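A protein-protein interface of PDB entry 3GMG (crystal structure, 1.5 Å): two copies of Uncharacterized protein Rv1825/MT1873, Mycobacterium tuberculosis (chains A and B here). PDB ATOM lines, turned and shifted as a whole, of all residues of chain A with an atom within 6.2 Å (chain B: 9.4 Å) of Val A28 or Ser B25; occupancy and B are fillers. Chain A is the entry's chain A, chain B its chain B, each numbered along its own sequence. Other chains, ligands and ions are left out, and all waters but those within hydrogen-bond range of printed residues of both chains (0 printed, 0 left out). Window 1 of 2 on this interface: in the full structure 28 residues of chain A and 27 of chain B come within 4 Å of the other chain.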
ATOM      1  N   ALA A  23     -18.362 -21.971  24.485  1.00  0.00           N
ATOM      2  CA  ALA A  23     -19.005 -21.696  25.773  1.00  0.00           C
ATOM      3  C   ALA A  23     -20.453 -21.257  25.566  1.00  0.00           C
ATOM      4  O   ALA A  23     -21.365 -21.800  26.188  1.00  0.00           O
ATOM      5  CB  ALA A  23     -18.235 -20.636  26.546  1.00  0.00           C
ATOM      6  N   LEU A  24     -20.650 -20.293  24.672  1.00  0.00           N
ATOM      7  CA  LEU A  24     -21.991 -19.809  24.317  1.00  0.00           C
ATOM      8  C   LEU A  24     -22.846 -20.946  23.778  1.00  0.00           C
ATOM      9  O   LEU A  24     -24.014 -21.090  24.154  1.00  0.00           O
ATOM     10  CB  LEU A  24     -21.886 -18.685  23.273  1.00  0.00           C
ATOM     11  CG  LEU A  24     -23.163 -17.986  22.795  1.00  0.00           C
ATOM     12  CD1 LEU A  24     -23.922 -17.307  23.938  1.00  0.00           C
ATOM     13  CD2 LEU A  24     -22.810 -16.965  21.706  1.00  0.00           C
ATOM     14  N   SER A  25     -22.257 -21.762  22.905  1.00  0.00           N
ATOM     15  CA  SER A  25     -22.993 -22.832  22.250  1.00  0.00           C
ATOM     16  C   SER A  25     -23.431 -23.885  23.254  1.00  0.00           C
ATOM     17  O   SER A  25     -24.537 -24.431  23.149  1.00  0.00           O
ATOM     18  CB  SER A  25     -22.162 -23.463  21.135  1.00  0.00           C
ATOM     19  OG  SER A  25     -21.957 -22.518  20.098  1.00  0.00           O
ATOM     20  N   ILE A  26     -22.590 -24.154  24.250  1.00  0.00           N
ATOM     21  CA  ILE A  26     -22.994 -25.078  25.314  1.00  0.00           C
ATOM     22  C   ILE A  26     -24.101 -24.471  26.167  1.00  0.00           C
ATOM     23  O   ILE A  26     -25.103 -25.136  26.452  1.00  0.00           O
ATOM     24  CB  ILE A  26     -21.817 -25.525  26.193  1.00  0.00           C
ATOM     25  CG1 ILE A  26     -20.877 -26.429  25.394  1.00  0.00           C
ATOM     26  CG2 ILE A  26     -22.349 -26.275  27.441  1.00  0.00           C
ATOM     27  CD1 ILE A  26     -19.566 -26.702  26.118  1.00  0.00           C
ATOM     28  N   LEU A  27     -23.929 -23.216  26.575  1.00  0.00           N
ATOM     29  CA  LEU A  27     -24.930 -22.518  27.401  1.00  0.00           C
ATOM     30  C   LEU A  27     -26.340 -22.591  26.816  1.00  0.00           C
ATOM     31  O   LEU A  27     -27.310 -22.874  27.509  1.00  0.00           O
ATOM     32  CB  LEU A  27     -24.540 -21.042  27.561  1.00  0.00           C
ATOM     33  CG  LEU A  27     -25.562 -20.117  28.223  1.00  0.00           C
ATOM     34  CD1 LEU A  27     -25.684 -20.462  29.688  1.00  0.00           C
ATOM     35  CD2 LEU A  27     -25.162 -18.650  28.009  1.00  0.00           C
ATOM     36  N   VAL A  28     -26.442 -22.318  25.524  1.00  0.00           N
ATOM     37  CA  VAL A  28     -27.740 -22.198  24.886  1.00  0.00           C
ATOM     38  C   VAL A  28     -28.253 -23.532  24.354  1.00  0.00           C
ATOM     39  O   VAL A  28     -29.372 -23.605  23.832  1.00  0.00           O
ATOM     40  CB  VAL A  28     -27.699 -21.098  23.801  1.00  0.00           C
ATOM     41  CG1 VAL A  28     -27.086 -19.831  24.382  1.00  0.00           C
ATOM     42  CG2 VAL A  28     -26.936 -21.565  22.568  1.00  0.00           C
ATOM     43  N   GLY A  29     -27.472 -24.599  24.532  1.00  0.00           N
ATOM     44  CA  GLY A  29     -27.878 -25.932  24.111  1.00  0.00           C
ATOM     45  C   GLY A  29     -27.737 -26.167  22.616  1.00  0.00           C
ATOM     46  O   GLY A  29     -28.388 -27.053  22.044  1.00  0.00           O
ATOM     47  N   ALA A  30     -26.854 -25.396  21.980  1.00  0.00           N
ATOM     48  CA  ALA A  30     -26.608 -25.536  20.538  1.00  0.00           C
ATOM     49  C   ALA A  30     -25.718 -26.727  20.181  1.00  0.00           C
ATOM     50  O   ALA A  30     -25.797 -27.253  19.061  1.00  0.00           O
ATOM     51  CB  ALA A  30     -25.990 -24.252  19.984  1.00  0.00           C
ATOM     52  N   VAL A  31     -24.856 -27.131  21.112  1.00  0.00           N
ATOM     53  CA  VAL A  31     -23.946 -28.253  20.910  1.00  0.00           C
ATOM     54  C   VAL A  31     -23.924 -29.114  22.164  1.00  0.00           C
ATOM     55  O   VAL A  31     -24.373 -28.699  23.241  1.00  0.00           O
ATOM     56  CB  VAL A  31     -22.522 -27.774  20.612  1.00  0.00           C
ATOM     57  CG1 VAL A  31     -22.514 -26.897  19.336  1.00  0.00           C
ATOM     58  CG2 VAL A  31     -21.937 -27.023  21.800  1.00  0.00           C
ATOM     59  N   ARG A  79     -32.796 -32.095  25.487  1.00  0.00           N
ATOM     60  CA  ARG A  79     -31.817 -31.188  26.063  1.00  0.00           C
ATOM     61  C   ARG A  79     -32.562 -30.109  26.811  1.00  0.00           C
ATOM     62  O   ARG A  79     -33.364 -29.384  26.229  1.00  0.00           O
ATOM     63  CB  ARG A  79     -30.980 -30.552  24.950  1.00  0.00           C
ATOM     64  CG  ARG A  79     -29.924 -29.564  25.457  1.00  0.00           C
ATOM     65  CD  ARG A  79     -28.874 -30.248  26.338  1.00  0.00           C
ATOM     66  NE  ARG A  79     -27.735 -29.370  26.607  1.00  0.00           N
ATOM     67  CZ  ARG A  79     -26.723 -29.145  25.780  1.00  0.00           C
ATOM     68  NH1 ARG A  79     -25.767 -28.275  26.139  1.00  0.00           N
ATOM     69  NH2 ARG A  79     -26.669 -29.740  24.592  1.00  0.00           N
ATOM     70  N   GLY A  81     -33.314 -26.648  28.616  1.00  0.00           N
ATOM     71  CA  GLY A  81     -32.917 -25.247  28.573  1.00  0.00           C
ATOM     72  C   GLY A  81     -33.760 -24.414  29.510  1.00  0.00           C
ATOM     73  O   GLY A  81     -34.644 -24.918  30.204  1.00  0.00           O
ATOM     74  N   ARG A 150     -30.915 -28.508  21.637  1.00  0.00           N
ATOM     75  CA  ARG A 150     -32.172 -27.770  21.642  1.00  0.00           C
ATOM     76  C   ARG A 150     -32.560 -27.350  20.238  1.00  0.00           C
ATOM     77  O   ARG A 150     -31.695 -27.098  19.400  1.00  0.00           O
ATOM     78  CB  ARG A 150     -32.067 -26.547  22.534  1.00  0.00           C
ATOM     79  CG  ARG A 150     -31.875 -26.911  23.979  1.00  0.00           C
ATOM     80  CD  ARG A 150     -32.441 -25.847  24.865  1.00  0.00           C
ATOM     81  NE  ARG A 150     -33.882 -26.017  25.047  1.00  0.00           N
ATOM     82  CZ  ARG A 150     -34.729 -25.039  25.338  1.00  0.00           C
ATOM     83  NH1 ARG A 150     -34.302 -23.776  25.445  1.00  0.00           N
ATOM     84  NH2 ARG A 150     -36.020 -25.323  25.494  1.00  0.00           N
ATOM     85  N   ALA B  19     -27.036 -20.214  12.548  1.00  0.00           N
ATOM     86  CA  ALA B  19     -28.334 -19.464  12.579  1.00  0.00           C
ATOM     87  C   ALA B  19     -29.284 -20.015  13.645  1.00  0.00           C
ATOM     88  O   ALA B  19     -30.174 -19.299  14.120  1.00  0.00           O
ATOM     89  CB  ALA B  19     -28.997 -19.494  11.208  1.00  0.00           C
ATOM     90  N   ARG B  20     -29.103 -21.283  14.013  1.00  0.00           N
ATOM     91  CA  ARG B  20     -29.792 -21.849  15.170  1.00  0.00           C
ATOM     92  C   ARG B  20     -29.198 -21.242  16.451  1.00  0.00           C
ATOM     93  O   ARG B  20     -29.899 -21.064  17.453  1.00  0.00           O
ATOM     94  CB  ARG B  20     -29.660 -23.377  15.190  1.00  0.00           C
ATOM     95  N   LEU B  21     -27.906 -20.922  16.398  1.00  0.00           N
ATOM     96  CA  LEU B  21     -27.189 -20.370  17.538  1.00  0.00           C
ATOM     97  C   LEU B  21     -27.720 -18.978  17.886  1.00  0.00           C
ATOM     98  O   LEU B  21     -27.856 -18.647  19.058  1.00  0.00           O
ATOM     99  CB  LEU B  21     -25.688 -20.309  17.241  1.00  0.00           C
ATOM    100  CG  LEU B  21     -24.764 -19.761  18.332  1.00  0.00           C
ATOM    101  CD1 LEU B  21     -24.816 -20.615  19.593  1.00  0.00           C
ATOM    102  CD2 LEU B  21     -23.335 -19.654  17.814  1.00  0.00           C
ATOM    103  N   ALA B  22     -28.028 -18.185  16.862  1.00  0.00           N
ATOM    104  CA  ALA B  22     -28.561 -16.836  17.059  1.00  0.00           C
ATOM    105  C   ALA B  22     -29.884 -16.853  17.809  1.00  0.00           C
ATOM    106  O   ALA B  22     -30.061 -16.123  18.793  1.00  0.00           O
ATOM    107  CB  ALA B  22     -28.728 -16.134  15.706  1.00  0.00           C
ATOM    108  N   ALA B  23     -30.816 -17.687  17.352  1.00  0.00           N
ATOM    109  CA  ALA B  23     -32.131 -17.766  17.966  1.00  0.00           C
ATOM    110  C   ALA B  23     -32.035 -18.217  19.424  1.00  0.00           C
ATOM    111  O   ALA B  23     -32.631 -17.609  20.317  1.00  0.00           O
ATOM    112  CB  ALA B  23     -33.053 -18.695  17.171  1.00  0.00           C
ATOM    113  N   LEU B  24     -31.267 -19.285  19.651  1.00  0.00           N
ATOM    114  CA  LEU B  24     -31.044 -19.802  20.998  1.00  0.00           C
ATOM    115  C   LEU B  24     -30.343 -18.755  21.870  1.00  0.00           C
ATOM    116  O   LEU B  24     -30.666 -18.595  23.050  1.00  0.00           O
ATOM    117  CB  LEU B  24     -30.215 -21.094  20.953  1.00  0.00           C
ATOM    118  CG  LEU B  24     -30.886 -22.323  20.331  1.00  0.00           C
ATOM    119  CD1 LEU B  24     -29.862 -23.420  20.061  1.00  0.00           C
ATOM    120  CD2 LEU B  24     -32.008 -22.822  21.230  1.00  0.00           C
ATOM    121  N   SER B  25     -29.399 -18.020  21.289  1.00  0.00           N
ATOM    122  CA  SER B  25     -28.678 -16.989  22.046  1.00  0.00           C
ATOM    123  C   SER B  25     -29.556 -15.791  22.439  1.00  0.00           C
ATOM    124  O   SER B  25     -29.400 -15.226  23.518  1.00  0.00           O
ATOM    125  CB  SER B  25     -27.461 -16.510  21.272  1.00  0.00           C
ATOM    126  OG  SER B  25     -26.491 -17.561  21.191  1.00  0.00           O
ATOM    127  N   ILE B  26     -30.472 -15.414  21.557  1.00  0.00           N
ATOM    128  CA  ILE B  26     -31.408 -14.338  21.875  1.00  0.00           C
ATOM    129  C   ILE B  26     -32.389 -14.761  22.963  1.00  0.00           C
ATOM    130  O   ILE B  26     -32.641 -13.997  23.906  1.00  0.00           O
ATOM    131  CB  ILE B  26     -32.139 -13.853  20.600  1.00  0.00           C
ATOM    132  CG1 ILE B  26     -31.165 -13.056  19.742  1.00  0.00           C
ATOM    133  CG2 ILE B  26     -33.333 -12.973  20.946  1.00  0.00           C
ATOM    134  CD1 ILE B  26     -31.648 -12.801  18.340  1.00  0.00           C
ATOM    135  N   LEU B  27     -32.916 -15.975  22.841  1.00  0.00           N
ATOM    136  CA  LEU B  27     -33.825 -16.513  23.852  1.00  0.00           C
ATOM    137  C   LEU B  27     -33.205 -16.501  25.244  1.00  0.00           C
ATOM    138  O   LEU B  27     -33.836 -16.058  26.206  1.00  0.00           O
ATOM    139  CB  LEU B  27     -34.213 -17.940  23.496  1.00  0.00           C
ATOM    140  CG  LEU B  27     -35.010 -18.688  24.570  1.00  0.00           C
ATOM    141  CD1 LEU B  27     -36.446 -18.213  24.593  1.00  0.00           C
ATOM    142  CD2 LEU B  27     -34.929 -20.187  24.318  1.00  0.00           C
ATOM    143  N   VAL B  28     -31.972 -16.992  25.351  1.00  0.00           N
ATOM    144  CA  VAL B  28     -31.288 -17.078  26.629  1.00  0.00           C
ATOM    145  C   VAL B  28     -30.784 -15.717  27.122  1.00  0.00           C
ATOM    146  O   VAL B  28     -30.394 -15.566  28.271  1.00  0.00           O
ATOM    147  CB  VAL B  28     -30.128 -18.106  26.528  1.00  0.00           C
ATOM    148  CG1 VAL B  28     -29.212 -18.039  27.744  1.00  0.00           C
ATOM    149  CG2 VAL B  28     -30.702 -19.505  26.380  1.00  0.00           C
ATOM    150  N   GLY B  29     -30.768 -14.723  26.236  1.00  0.00           N
ATOM    151  CA  GLY B  29     -30.322 -13.392  26.611  1.00  0.00           C
ATOM    152  C   GLY B  29     -28.820 -13.203  26.645  1.00  0.00           C
ATOM    153  O   GLY B  29     -28.319 -12.295  27.291  1.00  0.00           O
ATOM    154  N   ALA B  30     -28.104 -14.054  25.914  1.00  0.00           N
ATOM    155  CA  ALA B  30     -26.650 -14.030  25.893  1.00  0.00           C
ATOM    156  C   ALA B  30     -26.075 -13.131  24.812  1.00  0.00           C
ATOM    157  O   ALA B  30     -24.884 -12.811  24.830  1.00  0.00           O
ATOM    158  CB  ALA B  30     -26.110 -15.455  25.746  1.00  0.00           C
ATOM    159  N   VAL B  31     -26.921 -12.710  23.865  1.00  0.00           N
ATOM    160  CA  VAL B  31     -26.503 -11.723  22.864  1.00  0.00           C
ATOM    161  C   VAL B  31     -27.569 -10.633  22.776  1.00  0.00           C
ATOM    162  O   VAL B  31     -28.717 -10.868  23.149  1.00  0.00           O
ATOM    163  CB  VAL B  31     -26.259 -12.345  21.471  1.00  0.00           C
ATOM    164  CG1 VAL B  31     -25.153 -13.442  21.569  1.00  0.00           C
ATOM    165  CG2 VAL B  31     -27.544 -12.870  20.850  1.00  0.00           C
ATOM    166  N   GLY B  32     -27.176  -9.458  22.313  1.00  0.00           N
ATOM    167  CA  GLY B  32     -28.118  -8.357  22.105  1.00  0.00           C
ATOM    168  C   GLY B  32     -29.039  -8.662  20.943  1.00  0.00           C
ATOM    169  O   GLY B  32     -28.788  -9.541  20.107  1.00  0.00           O
ATOM    170  N   ALA B  33     -30.146  -7.942  20.906  1.00  0.00           N
ATOM    171  CA  ALA B  33     -31.136  -8.124  19.851  1.00  0.00           C
ATOM    172  C   ALA B  33     -31.653  -6.789  19.374  1.00  0.00           C
ATOM    173  O   ALA B  33     -31.651  -5.816  20.109  1.00  0.00           O
ATOM    174  CB  ALA B  33     -32.270  -9.011  20.333  1.00  0.00           C
ATOM    175  N   GLU B  67     -40.022 -11.105  21.830  1.00  0.00           N
ATOM    176  CA  GLU B  67     -38.924 -12.041  21.693  1.00  0.00           C
ATOM    177  C   GLU B  67     -37.673 -11.619  22.459  1.00  0.00           C
ATOM    178  O   GLU B  67     -36.753 -12.428  22.637  1.00  0.00           O
ATOM    179  CB  GLU B  67     -38.606 -12.257  20.202  1.00  0.00           C
ATOM    180  CG  GLU B  67     -39.749 -12.998  19.478  1.00  0.00           C
ATOM    181  CD  GLU B  67     -39.579 -13.092  17.981  1.00  0.00           C
ATOM    182  OE1 GLU B  67     -38.718 -12.407  17.428  1.00  0.00           O
ATOM    183  OE2 GLU B  67     -40.362 -13.864  17.387  1.00  0.00           O
ATOM    184  N   ALA B  68     -37.636 -10.377  22.938  1.00  0.00           N
ATOM    185  CA  ALA B  68     -36.576  -9.899  23.793  1.00  0.00           C
ATOM    186  C   ALA B  68     -37.147  -8.758  24.597  1.00  0.00           C
ATOM    187  O   ALA B  68     -37.919  -7.945  24.047  1.00  0.00           O
ATOM    188  CB  ALA B  68     -35.387  -9.455  22.976  1.00  0.00           C
ATOM    189  N   ARG B  79     -31.653  -7.520  31.318  1.00  0.00           N
ATOM    190  CA  ARG B  79     -32.193  -8.422  30.317  1.00  0.00           C
ATOM    191  C   ARG B  79     -33.099  -9.441  30.959  1.00  0.00           C
ATOM    192  O   ARG B  79     -32.703 -10.171  31.882  1.00  0.00           O
ATOM    193  CB  ARG B  79     -31.042  -9.107  29.550  1.00  0.00           C
ATOM    194  CG  ARG B  79     -31.454  -9.990  28.402  1.00  0.00           C
ATOM    195  CD  ARG B  79     -32.180  -9.198  27.310  1.00  0.00           C
ATOM    196  NE  ARG B  79     -32.358 -10.011  26.110  1.00  0.00           N
ATOM    197  CZ  ARG B  79     -31.415 -10.220  25.186  1.00  0.00           C
ATOM    198  NH1 ARG B  79     -30.226  -9.654  25.269  1.00  0.00           N
ATOM    199  NH2 ARG B  79     -31.689 -10.990  24.142  1.00  0.00           N
ATOM    200  N   VAL B  80     -34.339  -9.502  30.510  1.00  0.00           N
ATOM    201  CA  VAL B  80     -35.323 -10.352  31.066  1.00  0.00           C
ATOM    202  C   VAL B  80     -35.273 -11.708  30.395  1.00  0.00           C
ATOM    203  O   VAL B  80     -35.235 -11.821  29.171  1.00  0.00           O
ATOM    204  CB  VAL B  80     -36.723  -9.705  30.931  1.00  0.00           C
ATOM    205  CG1 VAL B  80     -37.799 -10.698  31.367  1.00  0.00           C
ATOM    206  CG2 VAL B  80     -36.754  -8.416  31.716  1.00  0.00           C
ATOM    207  N   VAL B 146     -32.286  -4.099  22.268  1.00  0.00           N
ATOM    208  CA  VAL B 146     -32.160  -4.750  23.556  1.00  0.00           C
ATOM    209  C   VAL B 146     -30.686  -5.168  23.702  1.00  0.00           C
ATOM    210  O   VAL B 146     -30.251  -6.180  23.151  1.00  0.00           O
ATOM    211  CB  VAL B 146     -33.142  -5.928  23.681  1.00  0.00           C
ATOM    212  CG1 VAL B 146     -32.851  -6.748  24.936  1.00  0.00           C
ATOM    213  CG2 VAL B 146     -34.599  -5.459  23.656  1.00  0.00           C
ATOM    214  N   ALA B 148     -28.846  -5.108  26.834  1.00  0.00           N
ATOM    215  CA  ALA B 148     -28.467  -5.738  28.080  1.00  0.00           C
ATOM    216  C   ALA B 148     -28.369  -7.227  27.878  1.00  0.00           C
ATOM    217  O   ALA B 148     -29.147  -7.814  27.126  1.00  0.00           O
ATOM    218  CB  ALA B 148     -29.458  -5.432  29.161  1.00  0.00           C
ATOM    219  N   LEU B 149     -27.431  -7.847  28.584  1.00  0.00           N
ATOM    220  CA  LEU B 149     -27.222  -9.287  28.508  1.00  0.00           C
ATOM    221  C   LEU B 149     -27.437  -9.882  29.886  1.00  0.00           C
ATOM    222  O   LEU B 149     -27.171  -9.223  30.894  1.00  0.00           O
ATOM    223  CB  LEU B 149     -25.782  -9.600  28.056  1.00  0.00           C
ATOM    224  CG  LEU B 149     -25.305  -8.951  26.770  1.00  0.00           C
ATOM    225  CD1 LEU B 149     -23.854  -9.333  26.497  1.00  0.00           C
ATOM    226  CD2 LEU B 149     -26.202  -9.370  25.608  1.00  0.00           C
ATOM    227  N   ARG B 150     -27.879 -11.126  29.932  1.00  0.00           N
ATOM    228  CA  ARG B 150     -28.001 -11.807  31.214  1.00  0.00           C
ATOM    229  C   ARG B 150     -26.623 -12.111  31.745  1.00  0.00           C
ATOM    230  O   ARG B 150     -25.684 -12.296  30.974  1.00  0.00           O
ATOM    231  CB  ARG B 150     -28.803 -13.060  31.068  1.00  0.00           C
ATOM    232  CG  ARG B 150     -30.245 -12.762  30.689  1.00  0.00           C
ATOM    233  CD  ARG B 150     -31.140 -13.888  31.081  1.00  0.00           C
ATOM    234  NE  ARG B 150     -31.523 -13.795  32.489  1.00  0.00           N
ATOM    235  CZ  ARG B 150     -32.179 -14.743  33.145  1.00  0.00           C
ATOM    236  NH1 ARG B 150     -32.475 -15.889  32.553  1.00  0.00           N
ATOM    237  NH2 ARG B 150     -32.518 -14.556  34.407  1.00  0.00           N
ATOM    238  N   HIS B 155     -18.277 -21.908  32.338  1.00  0.00           N
ATOM    239  CA  HIS B 155     -18.455 -23.298  32.701  1.00  0.00           C
ATOM    240  C   HIS B 155     -17.210 -23.817  33.396  1.00  0.00           C
ATOM    241  O   HIS B 155     -16.107 -23.757  32.840  1.00  0.00           O
ATOM    242  CB  HIS B 155     -18.688 -24.149  31.459  1.00  0.00           C
ATOM    243  CG  HIS B 155     -19.907 -23.755  30.699  1.00  0.00           C
ATOM    244  ND1 HIS B 155     -19.877 -23.356  29.377  1.00  0.00           N
ATOM    245  CD2 HIS B 155     -21.194 -23.654  31.102  1.00  0.00           C
ATOM    246  CE1 HIS B 155     -21.106 -23.046  28.998  1.00  0.00           C
ATOM    247  NE2 HIS B 155     -21.921 -23.216  30.024  1.00  0.00           N
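The backbone carbonyl oxygen of Ile A26 is in hydrogen-bond range of the guanidinium group of Arg A79 (3.2 Å).
N of Ala A30 lies within hydrogen-bond range of O of Ser A25.
O of Ser A25 is in hydrogen-bond range of N of Val A31 (3.4 Å).
The backbone NH (N) of Arg A150 sits at hydrogen-bond distance from the backbone carbonyl oxygen (O) of Gly A29.
The backbone carbonyl oxygen (O) of Leu B21 sits at hydrogen-bond distance from the side-chain hydroxyl (OG) of Ser B25 (2.8 Å).
O of Ser B25 is in hydrogen-bond range of N of Ala B30.
Of the printed residues of chain B, Val A28 touches Leu B21, Leu B24 and Ser B25.
Ser B25 touches two residues of chain A.
Leu A27 touches just one residue of chain B: His B155 (3.7 Å).
Gly A29 touches none of the printed residues of chain B.
Printed residues of chain B within 4 Å of Ala A23: His B155 (3.1 Å).
Of the printed residues of chain B, Leu A24 touches Ser B25 and Ala B30.
Printed residues of chain B within 4 Å of Ala A30: Leu B21 and Leu B24.
Printed residues of chain A within 4 Å of Leu B21: Ser A25, Val A28 and Ala A30.
Arg B20 touches none of the printed residues of chain A.
The nearest printed residue of chain A that does not touch Ser B25 is Ser A25 (6.2 Å).
Val A28 touches Leu B24, but with the chains exchanged Leu A24 does not touch Val B28 (6.6 Å).
Val A28 touches Ser B25, but with the chains exchanged Ser A25 does not touch Val B28 (8.5 Å).
Arg A150 touches Leu B24, but with the chains exchanged Leu A24 does not touch Arg B150 (8.8 Å).
Arg A150 touches Leu B27, but with the chains exchanged Leu A27 does not touch Arg B150 (7.0 Å).
Positions printed for both chains: 23, 24, 25, 26, 27, 28, 29, 30, 31, 79 and 150.
Of the 13 pairs that touch across the chains among the printed residues, 2 have their exchanged pair printed and touching as well.
OG of Ser B25 touches CG of Leu A24, at 3.7 Å.
Ser A25 touches Leu B21.
Ile A26 touches His B155.
N of Leu A27 touches CE1 of His B155, at 3.7 Å.
Leu B24 touches Val A28.
OG of Ser B25 touches CG1 of Val A28 (3.96 Å).
CB of Ala A30 touches CD1 of Leu B21, 3.8 Å away.
Ala A30 touches Leu B24 (CA to CD1, 3.9 Å).
Leu B24 touches Arg A150 (CD2 to CB, 3.9 Å).
Arg A150 touches Leu B27 (NH1 to CD2, 3.8 Å).
Hydrophobic or aromatic side chains of chain A within 4 Å of the printed part of chain B: Leu A24, Ile A26, Val A28 and Ala A30.
Hydrophobic or aromatic side chains of chain B within 4 Å of the printed part of chain A: Leu B21, Leu B24, Leu B27, Ala B30 and His B155.
Along chain B the printed residues that touch a printed residue of chain A span positions 21 to 155.
Among the printed residues, 13 pairs touch across the chains.
Among the printed residues, no Asp or Glu carboxylate lies within 4 Å of a Lys or Arg side-chain nitrogen of the other chain.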
